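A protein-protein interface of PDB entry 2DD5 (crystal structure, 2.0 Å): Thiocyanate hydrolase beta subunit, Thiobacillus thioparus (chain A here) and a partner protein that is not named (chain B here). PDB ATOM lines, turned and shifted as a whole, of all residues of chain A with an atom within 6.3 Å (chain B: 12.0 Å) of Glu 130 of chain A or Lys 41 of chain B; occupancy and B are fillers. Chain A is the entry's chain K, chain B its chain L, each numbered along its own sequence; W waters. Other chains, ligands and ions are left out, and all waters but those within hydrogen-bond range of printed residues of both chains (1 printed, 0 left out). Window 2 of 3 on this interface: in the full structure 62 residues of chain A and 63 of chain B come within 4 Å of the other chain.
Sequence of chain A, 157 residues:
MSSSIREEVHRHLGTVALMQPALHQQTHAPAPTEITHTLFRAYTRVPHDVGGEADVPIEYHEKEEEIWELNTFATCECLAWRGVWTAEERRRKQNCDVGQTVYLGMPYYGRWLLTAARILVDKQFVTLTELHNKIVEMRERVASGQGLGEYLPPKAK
Hydrophobic or aromatic side chains of chain A within 4 Å of the printed part of chain B: Phe 125, Val 126 and Leu 131. Among the printed residues, 9 pairs touch across the chains. Among the printed residues, Asp or Glu carboxylates within 4 Å of a Lys or Arg side-chain nitrogen of the other chain: Glu 130 of chain A with Lys 41 of chain B (2.7 Å), Lys 134 of chain A with Glu 36 of chain B (3.0 Å) and Lys 134 of chain A with Glu 40 of chain B (2.9 Å).
The side-chain carboxylate (OE1) of Glu 130 of chain A sits at hydrogen-bond distance from the backbone NH (N) of Thr 127 of chain A (2.8 Å). The backbone carbonyl oxygen (O) of Ala 38 of chain B is in hydrogen-bond range of the backbone NH (N) of Leu 43 of chain B (2.8 Å).
Water W1 bridges the side-chain carboxylate (OE1) of Glu 130 of chain A and the side-chain amino group (NZ) of Lys 41 of chain B.
Phe 125 of chain A touches Lys 41 of chain B. Leu 43 of chain B touches Phe 125 of chain A (CD2 to CD1, 3.7 Å). Lys 41 of chain B touches Val 126 of chain A (CG to CG1, 3.8 Å). CD1 of Leu 37 of chain B touches CD1 of Leu 131 of chain A, 3.8 Å away. Ala 33 of chain B touches Lys 134 of chain A (CB to CG, 3.4 Å). CD2 of Leu 37 of chain B touches CE of Lys 134 of chain A, 3.8 Å away.
OE1 of Glu 36 of chain B is in salt-bridge range of NZ of Lys 134 of chain A, 3.0 Å away. The side-chain amino group (NZ) of Lys 134 of chain A is in salt-bridge range of the side-chain carboxylate (OE2) of Glu 40 of chain B (2.9 Å). NZ of Lys 41 of chain B lies within salt-bridge range of OE2 of Glu 130 of chain A (2.7 Å).
Of the printed residues of chain B, Phe 125 of chain A touches Lys 41 and Leu 43. Val 126 of chain A touches just one residue of chain B: Lys 41 (3.8 Å). No residue of chain B comes within 4 Å of Thr 127 of chain A. No residue of chain B comes within 4 Å of Thr 129 of chain A. Leu 131 of chain A touches just one residue of chain B: Leu 37 (3.8 Å). No residue of chain B comes within 4 Å of His 132 of chain A. Asn 133 of chain A touches none of the printed residues of chain B. Of the printed residues of chain B, Lys 134 of chain A touches Ala 33 (3.4 Å), Glu 36 (3.0 Å), Leu 37 (3.8 Å) and Glu 40 (2.9 Å). Val 34 of chain B touches none of the printed residues of chain A. Of the printed residues of chain A, Leu 37 of chain B touches Leu 131 (3.8 Å) and Lys 134 (3.8 Å). Of chain A, only Phe 125, Val 126 and Glu 130 come within 4 Å of Lys 41 of chain B. Ser 45 of chain B touches none of the printed residues of chain A.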
ATOM      1  N   PHE A 125      22.446  24.196 -25.144  1.00  0.00           N
ATOM      2  CA  PHE A 125      22.892  25.123 -24.113  1.00  0.00           C
ATOM      3  C   PHE A 125      24.415  25.147 -24.144  1.00  0.00           C
ATOM      4  O   PHE A 125      25.045  26.120 -23.738  1.00  0.00           O
ATOM      5  CB  PHE A 125      22.356  24.708 -22.741  1.00  0.00           C
ATOM      6  CG  PHE A 125      20.884  24.973 -22.575  1.00  0.00           C
ATOM      7  CD1 PHE A 125      20.393  26.274 -22.619  1.00  0.00           C
ATOM      8  CD2 PHE A 125      19.986  23.922 -22.414  1.00  0.00           C
ATOM      9  CE1 PHE A 125      19.026  26.527 -22.509  1.00  0.00           C
ATOM     10  CE2 PHE A 125      18.616  24.164 -22.302  1.00  0.00           C
ATOM     11  CZ  PHE A 125      18.136  25.466 -22.351  1.00  0.00           C
ATOM     12  N   VAL A 126      24.996  24.059 -24.637  1.00  0.00           N
ATOM     13  CA  VAL A 126      26.442  23.945 -24.810  1.00  0.00           C
ATOM     14  C   VAL A 126      26.608  23.203 -26.126  1.00  0.00           C
ATOM     15  O   VAL A 126      25.761  22.386 -26.488  1.00  0.00           O
ATOM     16  CB  VAL A 126      27.130  23.108 -23.700  1.00  0.00           C
ATOM     17  CG1 VAL A 126      26.747  23.633 -22.327  1.00  0.00           C
ATOM     18  CG2 VAL A 126      26.758  21.640 -23.845  1.00  0.00           C
ATOM     19  N   THR A 127      27.675  23.491 -26.859  1.00  0.00           N
ATOM     20  CA  THR A 127      27.906  22.782 -28.107  1.00  0.00           C
ATOM     21  C   THR A 127      28.627  21.491 -27.728  1.00  0.00           C
ATOM     22  O   THR A 127      29.209  21.396 -26.643  1.00  0.00           O
ATOM     23  CB  THR A 127      28.812  23.587 -29.059  1.00  0.00           C
ATOM     24  OG1 THR A 127      30.072  23.824 -28.422  1.00  0.00           O
ATOM     25  CG2 THR A 127      28.159  24.928 -29.425  1.00  0.00           C
ATOM     26  N   LEU A 128      28.590  20.491 -28.601  1.00  0.00           N
ATOM     27  CA  LEU A 128      29.286  19.252 -28.291  1.00  0.00           C
ATOM     28  C   LEU A 128      30.774  19.579 -28.179  1.00  0.00           C
ATOM     29  O   LEU A 128      31.508  18.953 -27.416  1.00  0.00           O
ATOM     30  CB  LEU A 128      29.058  18.204 -29.383  1.00  0.00           C
ATOM     31  CG  LEU A 128      29.682  16.838 -29.080  1.00  0.00           C
ATOM     32  CD1 LEU A 128      29.157  16.321 -27.743  1.00  0.00           C
ATOM     33  CD2 LEU A 128      29.359  15.862 -30.200  1.00  0.00           C
ATOM     34  N   THR A 129      31.212  20.579 -28.940  1.00  0.00           N
ATOM     35  CA  THR A 129      32.612  20.987 -28.912  1.00  0.00           C
ATOM     36  C   THR A 129      32.980  21.481 -27.514  1.00  0.00           C
ATOM     37  O   THR A 129      34.035  21.128 -26.976  1.00  0.00           O
ATOM     38  CB  THR A 129      32.877  22.102 -29.938  1.00  0.00           C
ATOM     39  OG1 THR A 129      32.576  21.612 -31.251  1.00  0.00           O
ATOM     40  CG2 THR A 129      34.331  22.541 -29.891  1.00  0.00           C
ATOM     41  N   GLU A 130      32.106  22.293 -26.928  1.00  0.00           N
ATOM     42  CA  GLU A 130      32.334  22.813 -25.585  1.00  0.00           C
ATOM     43  C   GLU A 130      32.389  21.676 -24.566  1.00  0.00           C
ATOM     44  O   GLU A 130      33.191  21.709 -23.637  1.00  0.00           O
ATOM     45  CB  GLU A 130      31.228  23.801 -25.196  1.00  0.00           C
ATOM     46  CG  GLU A 130      31.283  25.130 -25.953  1.00  0.00           C
ATOM     47  CD  GLU A 130      30.168  26.084 -25.553  1.00  0.00           C
ATOM     48  OE1 GLU A 130      28.985  25.694 -25.652  1.00  0.00           O
ATOM     49  OE2 GLU A 130      30.473  27.226 -25.143  1.00  0.00           O
ATOM     50  N   LEU A 131      31.536  20.670 -24.738  1.00  0.00           N
ATOM     51  CA  LEU A 131      31.526  19.539 -23.813  1.00  0.00           C
ATOM     52  C   LEU A 131      32.825  18.749 -23.947  1.00  0.00           C
ATOM     53  O   LEU A 131      33.468  18.435 -22.951  1.00  0.00           O
ATOM     54  CB  LEU A 131      30.327  18.623 -24.090  1.00  0.00           C
ATOM     55  CG  LEU A 131      30.288  17.325 -23.281  1.00  0.00           C
ATOM     56  CD1 LEU A 131      30.310  17.632 -21.789  1.00  0.00           C
ATOM     57  CD2 LEU A 131      29.033  16.548 -23.648  1.00  0.00           C
ATOM     58  N   HIS A 132      33.201  18.435 -25.186  1.00  0.00           N
ATOM     59  CA  HIS A 132      34.435  17.702 -25.462  1.00  0.00           C
ATOM     60  C   HIS A 132      35.666  18.443 -24.940  1.00  0.00           C
ATOM     61  O   HIS A 132      36.582  17.830 -24.399  1.00  0.00           O
ATOM     62  CB  HIS A 132      34.597  17.472 -26.972  1.00  0.00           C
ATOM     63  CG  HIS A 132      33.720  16.388 -27.523  1.00  0.00           C
ATOM     64  ND1 HIS A 132      33.662  16.091 -28.868  1.00  0.00           N
ATOM     65  CD2 HIS A 132      32.884  15.516 -26.908  1.00  0.00           C
ATOM     66  CE1 HIS A 132      32.830  15.082 -29.059  1.00  0.00           C
ATOM     67  NE2 HIS A 132      32.343  14.714 -27.886  1.00  0.00           N
ATOM     68  N   ASN A 133      35.694  19.760 -25.121  1.00  0.00           N
ATOM     69  CA  ASN A 133      36.829  20.552 -24.658  1.00  0.00           C
ATOM     70  C   ASN A 133      36.882  20.599 -23.138  1.00  0.00           C
ATOM     71  O   ASN A 133      37.963  20.609 -22.549  1.00  0.00           O
ATOM     72  CB  ASN A 133      36.770  21.978 -25.226  1.00  0.00           C
ATOM     73  CG  ASN A 133      37.032  22.024 -26.727  1.00  0.00           C
ATOM     74  OD1 ASN A 133      37.657  21.126 -27.285  1.00  0.00           O
ATOM     75  ND2 ASN A 133      36.563  23.079 -27.381  1.00  0.00           N
ATOM     76  N   LYS A 134      35.718  20.631 -22.497  1.00  0.00           N
ATOM     77  CA  LYS A 134      35.678  20.663 -21.040  1.00  0.00           C
ATOM     78  C   LYS A 134      36.215  19.342 -20.496  1.00  0.00           C
ATOM     79  O   LYS A 134      36.939  19.318 -19.499  1.00  0.00           O
ATOM     80  CB  LYS A 134      34.244  20.911 -20.546  1.00  0.00           C
ATOM     81  CG  LYS A 134      34.080  20.844 -19.028  1.00  0.00           C
ATOM     82  CD  LYS A 134      34.877  21.922 -18.283  1.00  0.00           C
ATOM     83  CE  LYS A 134      34.219  23.294 -18.363  1.00  0.00           C
ATOM     84  NZ  LYS A 134      34.838  24.252 -17.389  1.00  0.00           N
ATOM     85  N   ILE A 135      35.875  18.238 -21.156  1.00  0.00           N
ATOM     86  CA  ILE A 135      36.360  16.934 -20.717  1.00  0.00           C
ATOM     87  C   ILE A 135      37.888  16.878 -20.840  1.00  0.00           C
ATOM     88  O   ILE A 135      38.576  16.368 -19.951  1.00  0.00           O
ATOM     89  CB  ILE A 135      35.719  15.799 -21.550  1.00  0.00           C
ATOM     90  CG1 ILE A 135      34.221  15.710 -21.223  1.00  0.00           C
ATOM     91  CG2 ILE A 135      36.421  14.477 -21.263  1.00  0.00           C
ATOM     92  CD1 ILE A 135      33.425  14.821 -22.171  1.00  0.00           C
ATOM     93  N   ILE B  29      35.075  12.656 -13.727  1.00  0.00           N
ATOM     94  CA  ILE B  29      35.517  13.667 -14.689  1.00  0.00           C
ATOM     95  C   ILE B  29      34.289  14.265 -15.381  1.00  0.00           C
ATOM     96  O   ILE B  29      34.126  15.486 -15.449  1.00  0.00           O
ATOM     97  CB  ILE B  29      36.433  13.045 -15.772  1.00  0.00           C
ATOM     98  CG1 ILE B  29      37.766  12.623 -15.155  1.00  0.00           C
ATOM     99  CG2 ILE B  29      36.648  14.035 -16.914  1.00  0.00           C
ATOM    100  CD1 ILE B  29      38.588  13.774 -14.637  1.00  0.00           C
ATOM    101  N   LEU B  30      33.424  13.393 -15.895  1.00  0.00           N
ATOM    102  CA  LEU B  30      32.224  13.835 -16.585  1.00  0.00           C
ATOM    103  C   LEU B  30      31.298  14.630 -15.670  1.00  0.00           C
ATOM    104  O   LEU B  30      30.704  15.615 -16.099  1.00  0.00           O
ATOM    105  CB  LEU B  30      31.480  12.631 -17.174  1.00  0.00           C
ATOM    106  CG  LEU B  30      30.230  12.938 -18.005  1.00  0.00           C
ATOM    107  CD1 LEU B  30      30.567  13.940 -19.108  1.00  0.00           C
ATOM    108  CD2 LEU B  30      29.685  11.643 -18.601  1.00  0.00           C
ATOM    109  N   GLU B  31      31.177  14.212 -14.410  1.00  0.00           N
ATOM    110  CA  GLU B  31      30.306  14.915 -13.461  1.00  0.00           C
ATOM    111  C   GLU B  31      30.776  16.364 -13.302  1.00  0.00           C
ATOM    112  O   GLU B  31      29.980  17.299 -13.409  1.00  0.00           O
ATOM    113  CB  GLU B  31      30.313  14.204 -12.101  1.00  0.00           C
ATOM    114  CG  GLU B  31      29.275  14.720 -11.083  1.00  0.00           C
ATOM    115  CD  GLU B  31      29.631  16.075 -10.473  1.00  0.00           C
ATOM    116  OE1 GLU B  31      30.752  16.216  -9.941  1.00  0.00           O
ATOM    117  OE2 GLU B  31      28.784  16.999 -10.514  1.00  0.00           O
ATOM    118  N   MET B  32      32.071  16.543 -13.050  1.00  0.00           N
ATOM    119  CA  MET B  32      32.647  17.880 -12.893  1.00  0.00           C
ATOM    120  C   MET B  32      32.425  18.727 -14.144  1.00  0.00           C
ATOM    121  O   MET B  32      32.054  19.899 -14.052  1.00  0.00           O
ATOM    122  CB  MET B  32      34.154  17.790 -12.621  1.00  0.00           C
ATOM    123  CG  MET B  32      34.533  17.428 -11.193  1.00  0.00           C
ATOM    124  SD  MET B  32      34.310  18.806 -10.039  1.00  0.00           S
ATOM    125  CE  MET B  32      35.792  19.779 -10.385  1.00  0.00           C
ATOM    126  N   ALA B  33      32.668  18.129 -15.307  1.00  0.00           N
ATOM    127  CA  ALA B  33      32.504  18.824 -16.579  1.00  0.00           C
ATOM    128  C   ALA B  33      31.076  19.319 -16.751  1.00  0.00           C
ATOM    129  O   ALA B  33      30.852  20.480 -17.081  1.00  0.00           O
ATOM    130  CB  ALA B  33      32.871  17.901 -17.734  1.00  0.00           C
ATOM    131  N   VAL B  34      30.111  18.430 -16.534  1.00  0.00           N
ATOM    132  CA  VAL B  34      28.705  18.791 -16.678  1.00  0.00           C
ATOM    133  C   VAL B  34      28.301  19.888 -15.698  1.00  0.00           C
ATOM    134  O   VAL B  34      27.644  20.855 -16.079  1.00  0.00           O
ATOM    135  CB  VAL B  34      27.787  17.552 -16.475  1.00  0.00           C
ATOM    136  CG1 VAL B  34      26.322  17.980 -16.387  1.00  0.00           C
ATOM    137  CG2 VAL B  34      27.963  16.591 -17.641  1.00  0.00           C
ATOM    138  N   ARG B  35      28.699  19.744 -14.438  1.00  0.00           N
ATOM    139  CA  ARG B  35      28.337  20.734 -13.432  1.00  0.00           C
ATOM    140  C   ARG B  35      28.945  22.105 -13.727  1.00  0.00           C
ATOM    141  O   ARG B  35      28.256  23.121 -13.641  1.00  0.00           O
ATOM    142  CB  ARG B  35      28.748  20.254 -12.037  1.00  0.00           C
ATOM    143  CG  ARG B  35      28.313  21.187 -10.911  1.00  0.00           C
ATOM    144  CD  ARG B  35      28.422  20.520  -9.552  1.00  0.00           C
ATOM    145  NE  ARG B  35      29.647  19.739  -9.446  1.00  0.00           N
ATOM    146  CZ  ARG B  35      30.182  19.323  -8.306  1.00  0.00           C
ATOM    147  NH1 ARG B  35      29.602  19.615  -7.150  1.00  0.00           N
ATOM    148  NH2 ARG B  35      31.298  18.607  -8.326  1.00  0.00           N
ATOM    149  N   GLU B  36      30.225  22.141 -14.082  1.00  0.00           N
ATOM    150  CA  GLU B  36      30.862  23.419 -14.382  1.00  0.00           C
ATOM    151  C   GLU B  36      30.227  24.091 -15.590  1.00  0.00           C
ATOM    152  O   GLU B  36      29.986  25.297 -15.573  1.00  0.00           O
ATOM    153  CB  GLU B  36      32.373  23.242 -14.591  1.00  0.00           C
ATOM    154  CG  GLU B  36      33.118  23.074 -13.273  1.00  0.00           C
ATOM    155  CD  GLU B  36      34.634  23.099 -13.415  1.00  0.00           C
ATOM    156  OE1 GLU B  36      35.141  23.460 -14.499  1.00  0.00           O
ATOM    157  OE2 GLU B  36      35.319  22.761 -12.426  1.00  0.00           O
ATOM    158  N   LEU B  37      29.940  23.314 -16.634  1.00  0.00           N
ATOM    159  CA  LEU B  37      29.311  23.873 -17.825  1.00  0.00           C
ATOM    160  C   LEU B  37      27.921  24.428 -17.514  1.00  0.00           C
ATOM    161  O   LEU B  37      27.564  25.520 -17.959  1.00  0.00           O
ATOM    162  CB  LEU B  37      29.204  22.811 -18.923  1.00  0.00           C
ATOM    163  CG  LEU B  37      30.511  22.456 -19.645  1.00  0.00           C
ATOM    164  CD1 LEU B  37      30.283  21.267 -20.563  1.00  0.00           C
ATOM    165  CD2 LEU B  37      31.004  23.665 -20.438  1.00  0.00           C
ATOM    166  N   ALA B  38      27.136  23.680 -16.744  1.00  0.00           N
ATOM    167  CA  ALA B  38      25.788  24.120 -16.403  1.00  0.00           C
ATOM    168  C   ALA B  38      25.834  25.442 -15.641  1.00  0.00           C
ATOM    169  O   ALA B  38      25.033  26.346 -15.893  1.00  0.00           O
ATOM    170  CB  ALA B  38      25.077  23.053 -15.567  1.00  0.00           C
ATOM    171  N   ILE B  39      26.777  25.551 -14.712  1.00  0.00           N
ATOM    172  CA  ILE B  39      26.916  26.768 -13.922  1.00  0.00           C
ATOM    173  C   ILE B  39      27.448  27.912 -14.787  1.00  0.00           C
ATOM    174  O   ILE B  39      26.946  29.037 -14.718  1.00  0.00           O
ATOM    175  CB  ILE B  39      27.839  26.527 -12.710  1.00  0.00           C
ATOM    176  CG1 ILE B  39      27.154  25.555 -11.740  1.00  0.00           C
ATOM    177  CG2 ILE B  39      28.160  27.853 -12.013  1.00  0.00           C
ATOM    178  CD1 ILE B  39      27.991  25.169 -10.536  1.00  0.00           C
ATOM    179  N   GLU B  40      28.448  27.622 -15.616  1.00  0.00           N
ATOM    180  CA  GLU B  40      29.013  28.637 -16.496  1.00  0.00           C
ATOM    181  C   GLU B  40      27.973  29.176 -17.475  1.00  0.00           C
ATOM    182  O   GLU B  40      27.988  30.361 -17.810  1.00  0.00           O
ATOM    183  CB  GLU B  40      30.205  28.064 -17.268  1.00  0.00           C
ATOM    184  CG  GLU B  40      31.474  27.937 -16.434  1.00  0.00           C
ATOM    185  CD  GLU B  40      32.534  27.070 -17.100  1.00  0.00           C
ATOM    186  OE1 GLU B  40      32.436  26.838 -18.327  1.00  0.00           O
ATOM    187  OE2 GLU B  40      33.470  26.631 -16.395  1.00  0.00           O
ATOM    188  N   LYS B  41      27.066  28.313 -17.929  1.00  0.00           N
ATOM    189  CA  LYS B  41      26.033  28.733 -18.873  1.00  0.00           C
ATOM    190  C   LYS B  41      24.809  29.326 -18.175  1.00  0.00           C
ATOM    191  O   LYS B  41      23.854  29.742 -18.832  1.00  0.00           O
ATOM    192  CB  LYS B  41      25.604  27.551 -19.755  1.00  0.00           C
ATOM    193  CG  LYS B  41      26.696  27.022 -20.678  1.00  0.00           C
ATOM    194  CD  LYS B  41      27.156  28.092 -21.664  1.00  0.00           C
ATOM    195  CE  LYS B  41      28.232  27.557 -22.590  1.00  0.00           C
ATOM    196  NZ  LYS B  41      28.686  28.593 -23.562  1.00  0.00           N
ATOM    197  N   GLY B  42      24.844  29.359 -16.846  1.00  0.00           N
ATOM    198  CA  GLY B  42      23.736  29.909 -16.082  1.00  0.00           C
ATOM    199  C   GLY B  42      22.473  29.061 -16.068  1.00  0.00           C
ATOM    200  O   GLY B  42      21.378  29.592 -15.866  1.00  0.00           O
ATOM    201  N   LEU B  43      22.606  27.753 -16.280  1.00  0.00           N
ATOM    202  CA  LEU B  43      21.441  26.860 -16.278  1.00  0.00           C
ATOM    203  C   LEU B  43      20.911  26.743 -14.846  1.00  0.00           C
ATOM    204  O   LEU B  43      19.702  26.743 -14.617  1.00  0.00           O
ATOM    205  CB  LEU B  43      21.827  25.496 -16.853  1.00  0.00           C
ATOM    206  CG  LEU B  43      22.444  25.621 -18.254  1.00  0.00           C
ATOM    207  CD1 LEU B  43      22.638  24.242 -18.850  1.00  0.00           C
ATOM    208  CD2 LEU B  43      21.547  26.465 -19.158  1.00  0.00           C
ATOM    209  N   PHE B  44      21.825  26.615 -13.893  1.00  0.00           N
ATOM    210  CA  PHE B  44      21.481  26.606 -12.476  1.00  0.00           C
ATOM    211  C   PHE B  44      22.719  27.153 -11.781  1.00  0.00           C
ATOM    212  O   PHE B  44      23.807  27.140 -12.356  1.00  0.00           O
ATOM    213  CB  PHE B  44      21.065  25.212 -11.954  1.00  0.00           C
ATOM    214  CG  PHE B  44      22.140  24.162 -12.012  1.00  0.00           C
ATOM    215  CD1 PHE B  44      23.205  24.173 -11.114  1.00  0.00           C
ATOM    216  CD2 PHE B  44      22.050  23.120 -12.934  1.00  0.00           C
ATOM    217  CE1 PHE B  44      24.163  23.162 -11.131  1.00  0.00           C
ATOM    218  CE2 PHE B  44      23.005  22.101 -12.957  1.00  0.00           C
ATOM    219  CZ  PHE B  44      24.063  22.123 -12.052  1.00  0.00           C
ATOM    220  N   SER B  45      22.559  27.661 -10.567  1.00  0.00           N
ATOM    221  CA  SER B  45      23.684  28.253  -9.855  1.00  0.00           C
ATOM    222  C   SER B  45      24.406  27.298  -8.917  1.00  0.00           C
ATOM    223  O   SER B  45      23.915  26.209  -8.610  1.00  0.00           O
ATOM    224  CB  SER B  45      23.201  29.470  -9.059  1.00  0.00           C
ATOM    225  OG  SER B  45      22.318  29.069  -8.026  1.00  0.00           O
ATOM    226  N   ALA B  46      25.586  27.715  -8.466  1.00  0.00           N
ATOM    227  CA  ALA B  46      26.360  26.913  -7.529  1.00  0.00           C
ATOM    228  C   ALA B  46      25.508  26.788  -6.267  1.00  0.00           C
ATOM    229  O   ALA B  46      25.472  25.733  -5.631  1.00  0.00           O
ATOM    230  CB  ALA B  46      27.684  27.599  -7.206  1.00  0.00           C
ATOM    231  N   ASP B  48      22.206  26.806  -6.076  1.00  0.00           N
ATOM    232  CA  ASP B  48      21.144  25.830  -6.336  1.00  0.00           C
ATOM    233  C   ASP B  48      21.620  24.413  -6.051  1.00  0.00           C
ATOM    234  O   ASP B  48      20.938  23.634  -5.386  1.00  0.00           O
ATOM    235  CB  ASP B  48      20.693  25.860  -7.804  1.00  0.00           C
ATOM    236  CG  ASP B  48      19.937  27.113  -8.171  1.00  0.00           C
ATOM    237  OD1 ASP B  48      19.429  27.802  -7.258  1.00  0.00           O
ATOM    238  OD2 ASP B  48      19.838  27.396  -9.387  1.00  0.00           O
HETATM  239  O   HOH W   1      27.143  27.352 -26.369  1.00  0.00           O
